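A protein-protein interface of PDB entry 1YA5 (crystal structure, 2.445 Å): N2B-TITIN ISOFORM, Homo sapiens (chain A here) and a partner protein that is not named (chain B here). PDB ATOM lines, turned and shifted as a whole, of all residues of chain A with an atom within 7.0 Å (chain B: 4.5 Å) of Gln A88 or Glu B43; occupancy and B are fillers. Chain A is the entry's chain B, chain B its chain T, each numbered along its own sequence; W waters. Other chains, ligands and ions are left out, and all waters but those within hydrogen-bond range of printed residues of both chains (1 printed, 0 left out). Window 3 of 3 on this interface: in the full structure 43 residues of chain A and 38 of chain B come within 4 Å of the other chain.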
ATOM      1  N   ALA A   5      14.365 -22.516 -24.437  1.00  0.00           N
ATOM      2  CA  ALA A   5      14.916 -21.974 -23.196  1.00  0.00           C
ATOM      3  C   ALA A   5      14.371 -22.735 -22.003  1.00  0.00           C
ATOM      4  O   ALA A   5      13.246 -23.241 -22.034  1.00  0.00           O
ATOM      5  CB  ALA A   5      14.614 -20.502 -23.065  1.00  0.00           C
ATOM      6  N   PRO A   6      15.173 -22.804 -20.936  1.00  0.00           N
ATOM      7  CA  PRO A   6      14.826 -23.614 -19.783  1.00  0.00           C
ATOM      8  C   PRO A   6      13.644 -23.014 -19.053  1.00  0.00           C
ATOM      9  O   PRO A   6      13.585 -21.804 -18.837  1.00  0.00           O
ATOM     10  CB  PRO A   6      16.075 -23.537 -18.911  1.00  0.00           C
ATOM     11  CG  PRO A   6      17.154 -22.942 -19.794  1.00  0.00           C
ATOM     12  CD  PRO A   6      16.444 -22.081 -20.749  1.00  0.00           C
ATOM     13  N   THR A   7      12.694 -23.864 -18.709  1.00  0.00           N
ATOM     14  CA  THR A   7      11.575 -23.468 -17.890  1.00  0.00           C
ATOM     15  C   THR A   7      11.436 -24.481 -16.758  1.00  0.00           C
ATOM     16  O   THR A   7      11.743 -25.661 -16.935  1.00  0.00           O
ATOM     17  CB  THR A   7      10.292 -23.426 -18.724  1.00  0.00           C
ATOM     18  OG1 THR A   7       9.209 -22.923 -17.923  1.00  0.00           O
ATOM     19  CG2 THR A   7       9.937 -24.824 -19.215  1.00  0.00           C
ATOM     20  N   PHE A   8      10.991 -24.020 -15.593  1.00  0.00           N
ATOM     21  CA  PHE A   8      10.755 -24.909 -14.454  1.00  0.00           C
ATOM     22  C   PHE A   8       9.375 -25.512 -14.582  1.00  0.00           C
ATOM     23  O   PHE A   8       8.383 -24.799 -14.530  1.00  0.00           O
ATOM     24  CB  PHE A   8      10.866 -24.141 -13.127  1.00  0.00           C
ATOM     25  CG  PHE A   8      12.287 -23.841 -12.699  1.00  0.00           C
ATOM     26  CD1 PHE A   8      12.915 -22.676 -13.093  1.00  0.00           C
ATOM     27  CD2 PHE A   8      12.985 -24.722 -11.892  1.00  0.00           C
ATOM     28  CE1 PHE A   8      14.218 -22.399 -12.708  1.00  0.00           C
ATOM     29  CE2 PHE A   8      14.278 -24.444 -11.485  1.00  0.00           C
ATOM     30  CZ  PHE A   8      14.899 -23.280 -11.899  1.00  0.00           C
ATOM     31  N   GLU A  36      22.779 -25.840 -18.281  1.00  0.00           N
ATOM     32  CA  GLU A  36      23.791 -25.858 -17.233  1.00  0.00           C
ATOM     33  C   GLU A  36      23.132 -25.372 -15.968  1.00  0.00           C
ATOM     34  O   GLU A  36      22.583 -24.276 -15.925  1.00  0.00           O
ATOM     35  CB  GLU A  36      24.957 -24.920 -17.565  1.00  0.00           C
ATOM     36  CG  GLU A  36      25.780 -25.325 -18.783  1.00  0.00           C
ATOM     37  CD  GLU A  36      26.581 -26.600 -18.561  1.00  0.00           C
ATOM     38  OE1 GLU A  36      27.112 -26.780 -17.439  1.00  0.00           O
ATOM     39  OE2 GLU A  36      26.685 -27.416 -19.511  1.00  0.00           O
ATOM     40  N   LYS A  81      19.563 -22.260 -10.646  1.00  0.00           N
ATOM     41  CA  LYS A  81      19.690 -21.508 -11.883  1.00  0.00           C
ATOM     42  C   LYS A  81      19.958 -22.434 -13.061  1.00  0.00           C
ATOM     43  O   LYS A  81      20.830 -23.289 -12.992  1.00  0.00           O
ATOM     44  CB  LYS A  81      20.830 -20.502 -11.755  1.00  0.00           C
ATOM     45  CG  LYS A  81      20.801 -19.419 -12.797  1.00  0.00           C
ATOM     46  CD  LYS A  81      22.199 -18.870 -13.031  1.00  0.00           C
ATOM     47  CE  LYS A  81      22.516 -17.674 -12.128  1.00  0.00           C
ATOM     48  NZ  LYS A  81      23.576 -16.807 -12.749  1.00  0.00           N
ATOM     49  N   ALA A  82      19.198 -22.261 -14.139  1.00  0.00           N
ATOM     50  CA  ALA A  82      19.349 -23.072 -15.351  1.00  0.00           C
ATOM     51  C   ALA A  82      19.575 -22.196 -16.585  1.00  0.00           C
ATOM     52  O   ALA A  82      18.746 -21.348 -16.918  1.00  0.00           O
ATOM     53  CB  ALA A  82      18.137 -23.975 -15.558  1.00  0.00           C
ATOM     54  N   THR A  83      20.693 -22.423 -17.268  1.00  0.00           N
ATOM     55  CA  THR A  83      21.097 -21.587 -18.381  1.00  0.00           C
ATOM     56  C   THR A  83      21.320 -22.455 -19.591  1.00  0.00           C
ATOM     57  O   THR A  83      21.754 -23.592 -19.476  1.00  0.00           O
ATOM     58  CB  THR A  83      22.409 -20.882 -18.053  1.00  0.00           C
ATOM     59  OG1 THR A  83      22.345 -20.340 -16.727  1.00  0.00           O
ATOM     60  CG2 THR A  83      22.651 -19.747 -19.020  1.00  0.00           C
ATOM     61  N   ASN A  84      21.013 -21.927 -20.762  1.00  0.00           N
ATOM     62  CA  ASN A  84      21.456 -22.546 -22.003  1.00  0.00           C
ATOM     63  C   ASN A  84      21.446 -21.509 -23.109  1.00  0.00           C
ATOM     64  O   ASN A  84      21.293 -20.320 -22.829  1.00  0.00           O
ATOM     65  CB  ASN A  84      20.613 -23.780 -22.346  1.00  0.00           C
ATOM     66  CG  ASN A  84      19.253 -23.432 -22.886  1.00  0.00           C
ATOM     67  OD1 ASN A  84      18.995 -22.293 -23.263  1.00  0.00           O
ATOM     68  ND2 ASN A  84      18.366 -24.421 -22.933  1.00  0.00           N
ATOM     69  N   GLY A  85      21.632 -21.946 -24.351  1.00  0.00           N
ATOM     70  CA  GLY A  85      21.673 -21.033 -25.489  1.00  0.00           C
ATOM     71  C   GLY A  85      20.478 -20.095 -25.600  1.00  0.00           C
ATOM     72  O   GLY A  85      20.621 -18.940 -26.010  1.00  0.00           O
ATOM     73  N   SER A  86      19.294 -20.581 -25.231  1.00  0.00           N
ATOM     74  CA  SER A  86      18.053 -19.848 -25.479  1.00  0.00           C
ATOM     75  C   SER A  86      17.609 -18.956 -24.318  1.00  0.00           C
ATOM     76  O   SER A  86      16.707 -18.126 -24.459  1.00  0.00           O
ATOM     77  CB  SER A  86      16.942 -20.822 -25.858  1.00  0.00           C
ATOM     78  OG  SER A  86      17.268 -21.477 -27.069  1.00  0.00           O
ATOM     79  N   GLY A  87      18.248 -19.134 -23.170  1.00  0.00           N
ATOM     80  CA  GLY A  87      18.025 -18.252 -22.041  1.00  0.00           C
ATOM     81  C   GLY A  87      18.329 -18.903 -20.715  1.00  0.00           C
ATOM     82  O   GLY A  87      19.212 -19.737 -20.606  1.00  0.00           O
ATOM     83  N   GLN A  88      17.572 -18.516 -19.699  1.00  0.00           N
ATOM     84  CA  GLN A  88      17.918 -18.802 -18.323  1.00  0.00           C
ATOM     85  C   GLN A  88      16.660 -18.790 -17.469  1.00  0.00           C
ATOM     86  O   GLN A  88      15.686 -18.130 -17.791  1.00  0.00           O
ATOM     87  CB  GLN A  88      18.868 -17.731 -17.832  1.00  0.00           C
ATOM     88  CG  GLN A  88      19.730 -18.129 -16.668  1.00  0.00           C
ATOM     89  CD  GLN A  88      20.379 -16.923 -16.044  1.00  0.00           C
ATOM     90  OE1 GLN A  88      21.124 -17.026 -15.060  1.00  0.00           O
ATOM     91  NE2 GLN A  88      20.091 -15.750 -16.613  1.00  0.00           N
ATOM     92  N   ALA A  89      16.678 -19.534 -16.373  1.00  0.00           N
ATOM     93  CA  ALA A  89      15.550 -19.569 -15.455  1.00  0.00           C
ATOM     94  C   ALA A  89      16.121 -19.703 -14.069  1.00  0.00           C
ATOM     95  O   ALA A  89      17.135 -20.368 -13.873  1.00  0.00           O
ATOM     96  CB  ALA A  89      14.651 -20.753 -15.766  1.00  0.00           C
ATOM     97  N   THR A  90      15.478 -19.067 -13.107  1.00  0.00           N
ATOM     98  CA  THR A  90      15.950 -19.108 -11.738  1.00  0.00           C
ATOM     99  C   THR A  90      14.778 -19.334 -10.808  1.00  0.00           C
ATOM    100  O   THR A  90      13.738 -18.679 -10.930  1.00  0.00           O
ATOM    101  CB  THR A  90      16.671 -17.785 -11.344  1.00  0.00           C
ATOM    102  OG1 THR A  90      17.590 -17.414 -12.373  1.00  0.00           O
ATOM    103  CG2 THR A  90      17.471 -17.973 -10.078  1.00  0.00           C
ATOM    104  N   HIS B  41      12.124 -16.523 -11.858  1.00  0.00           N
ATOM    105  CA  HIS B  41      12.121 -15.744 -13.083  1.00  0.00           C
ATOM    106  C   HIS B  41      12.832 -16.486 -14.168  1.00  0.00           C
ATOM    107  O   HIS B  41      13.817 -17.155 -13.911  1.00  0.00           O
ATOM    108  CB  HIS B  41      12.673 -14.324 -12.901  1.00  0.00           C
ATOM    109  CG  HIS B  41      14.077 -14.273 -12.404  1.00  0.00           C
ATOM    110  ND1 HIS B  41      14.457 -13.483 -11.340  1.00  0.00           N
ATOM    111  CD2 HIS B  41      15.200 -14.901 -12.826  1.00  0.00           C
ATOM    112  CE1 HIS B  41      15.755 -13.630 -11.124  1.00  0.00           C
ATOM    113  NE2 HIS B  41      16.231 -14.484 -12.014  1.00  0.00           N
ATOM    114  N   GLU B  42      12.292 -16.373 -15.377  1.00  0.00           N
ATOM    115  CA  GLU B  42      12.745 -17.106 -16.538  1.00  0.00           C
ATOM    116  C   GLU B  42      12.910 -16.102 -17.673  1.00  0.00           C
ATOM    117  O   GLU B  42      11.967 -15.391 -17.972  1.00  0.00           O
ATOM    118  CB  GLU B  42      11.675 -18.133 -16.934  1.00  0.00           C
ATOM    119  CG  GLU B  42      11.126 -18.970 -15.784  1.00  0.00           C
ATOM    120  CD  GLU B  42      10.441 -20.248 -16.268  1.00  0.00           C
ATOM    121  OE1 GLU B  42      10.068 -20.320 -17.451  1.00  0.00           O
ATOM    122  OE2 GLU B  42      10.262 -21.193 -15.475  1.00  0.00           O
ATOM    123  N   GLU B  43      14.092 -16.031 -18.290  1.00  0.00           N
ATOM    124  CA  GLU B  43      14.288 -15.223 -19.503  1.00  0.00           C
ATOM    125  C   GLU B  43      14.490 -16.061 -20.766  1.00  0.00           C
ATOM    126  O   GLU B  43      15.479 -16.773 -20.890  1.00  0.00           O
ATOM    127  CB  GLU B  43      15.479 -14.281 -19.350  1.00  0.00           C
ATOM    128  CG  GLU B  43      15.306 -13.252 -18.261  1.00  0.00           C
ATOM    129  CD  GLU B  43      15.206 -13.912 -16.909  1.00  0.00           C
ATOM    130  OE1 GLU B  43      16.084 -14.777 -16.655  1.00  0.00           O
ATOM    131  OE2 GLU B  43      14.255 -13.593 -16.125  1.00  0.00           O
ATOM    132  N   ASP B  44      13.559 -15.958 -21.707  1.00  0.00           N
ATOM    133  CA  ASP B  44      13.698 -16.587 -23.013  1.00  0.00           C
ATOM    134  C   ASP B  44      14.282 -15.590 -24.000  1.00  0.00           C
ATOM    135  O   ASP B  44      13.541 -14.826 -24.610  1.00  0.00           O
ATOM    136  CB  ASP B  44      12.329 -17.009 -23.518  1.00  0.00           C
ATOM    137  CG  ASP B  44      12.409 -18.060 -24.585  1.00  0.00           C
ATOM    138  OD1 ASP B  44      13.172 -17.884 -25.559  1.00  0.00           O
ATOM    139  OD2 ASP B  44      11.712 -19.083 -24.456  1.00  0.00           O
ATOM    140  N   THR B  45      15.601 -15.595 -24.158  1.00  0.00           N
ATOM    141  CA  THR B  45      16.276 -14.580 -24.967  1.00  0.00           C
ATOM    142  C   THR B  45      16.168 -14.894 -26.453  1.00  0.00           C
ATOM    143  O   THR B  45      16.543 -14.088 -27.313  1.00  0.00           O
ATOM    144  CB  THR B  45      17.756 -14.471 -24.612  1.00  0.00           C
ATOM    145  OG1 THR B  45      18.245 -15.766 -24.236  1.00  0.00           O
ATOM    146  CG2 THR B  45      17.958 -13.508 -23.449  1.00  0.00           C
ATOM    147  N   GLU B  49      10.838 -13.324 -24.301  1.00  0.00           N
ATOM    148  CA  GLU B  49       9.782 -13.458 -23.315  1.00  0.00           C
ATOM    149  C   GLU B  49      10.376 -13.616 -21.915  1.00  0.00           C
ATOM    150  O   GLU B  49      11.334 -14.366 -21.713  1.00  0.00           O
ATOM    151  CB  GLU B  49       8.889 -14.632 -23.680  1.00  0.00           C
ATOM    152  CG  GLU B  49       8.207 -14.493 -25.027  1.00  0.00           C
ATOM    153  CD  GLU B  49       7.671 -15.817 -25.545  1.00  0.00           C
ATOM    154  OE1 GLU B  49       7.170 -15.868 -26.691  1.00  0.00           O
ATOM    155  OE2 GLU B  49       7.743 -16.814 -24.802  1.00  0.00           O
ATOM    156  N   THR B  50       9.833 -12.874 -20.953  1.00  0.00           N
ATOM    157  CA  THR B  50      10.293 -12.982 -19.583  1.00  0.00           C
ATOM    158  C   THR B  50       9.095 -13.269 -18.713  1.00  0.00           C
ATOM    159  O   THR B  50       7.987 -12.836 -19.008  1.00  0.00           O
ATOM    160  CB  THR B  50      10.912 -11.695 -19.128  1.00  0.00           C
ATOM    161  OG1 THR B  50       9.887 -10.714 -19.022  1.00  0.00           O
ATOM    162  CG2 THR B  50      11.885 -11.200 -20.156  1.00  0.00           C
HETATM  163  O   HOH W   1      16.655 -16.531 -14.587  1.00  0.00           O
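The backbone NH (N) of Asp B44 lies within hydrogen-bond range of the backbone carbonyl oxygen (O) of Glu B49. The backbone NH of Ala A89 is in hydrogen-bond range of the backbone carbonyl oxygen of Ala A82 (2.8 Å). N of Ser A86 is in hydrogen-bond range of OD1 of Asn A84, 2.6 Å away. The side-chain amide oxygen (OD1) of Asn A84 sits at hydrogen-bond distance from the backbone NH (N) of Gly A87, at 3.2 Å. OE1 of Gln A88 lies close to NZ of Lys A81 (3.4 Å).
CB of Ala A5 touches OD2 of Asp B44 (3.5 Å). O of Ser A86 touches C of Asp B44, 3.5 Å away. O of Glu B43 touches CA of Gly A87, 3.2 Å away. OG1 of Thr B45 touches CA of Gly A87, 3.3 Å away. Gln A88 touches Glu B42 (O to CA, 3.4 Å). Ala A89 touches His B41 (CA to O, 3.3 Å). Glu B42 touches Ala A89.
Of chain B, only Glu B42 (3.4 Å) and Glu B43 (2.7 Å) come within 4 Å of Gln A88. Of the printed residues of chain A, Glu B43 touches Gly A87 and Gln A88. Printed residues of chain B within 4 Å of Phe A8: Glu B42. Of the printed residues of chain A, Glu B42 touches Thr A7 (2.8 Å), Phe A8 (2.9 Å), Gln A88 (3.4 Å) and Ala A89 (3.9 Å). The nearest printed residue of chain B that does not touch Ala A5 is Glu B43 (4.4 Å).
Of the 7 printed residues of chain B, 5 touch a printed residue of chain A. Hydrophobic or aromatic side chains of chain B within 4 Å of the printed part of chain A: His B41. Printed residues of chain A that touch a printed residue of chain B: Ala A5, Thr A7, Phe A8, Ser A86, Gly A87, Gln A88, Ala A89 and Thr A90. Among the printed residues, 12 pairs touch across the chains. Among the printed residues, no Asp or Glu carboxylate lies within 4 Å of a Lys or Arg side-chain nitrogen of the other chain.
The side-chain carboxylate (OE2) of Glu B42 is in hydrogen-bond range of the backbone NH (N) of Phe A8 (2.9 Å). The side-chain hydroxyl (OG1) of Thr A7 is in hydrogen-bond range of the side-chain carboxylate (OE1) of Glu B42 (2.8 Å). The backbone NH (N) of Thr A90 sits at hydrogen-bond distance from the backbone carbonyl oxygen (O) of His B41 (2.7 Å). The backbone NH (N) of Glu B43 is in hydrogen-bond range of the backbone carbonyl oxygen (O) of Gln A88, 2.7 Å away. The backbone carbonyl oxygen (O) of Ser A86 lies within hydrogen-bond range of the backbone NH (N) of Thr B45.
Water W1 lies within hydrogen-bond range of the side-chain hydroxyl of Thr A90, the side-chain carboxylate of Glu B43, the backbone carbonyl oxygen of His B41 and the backbone NH of Ala A89.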
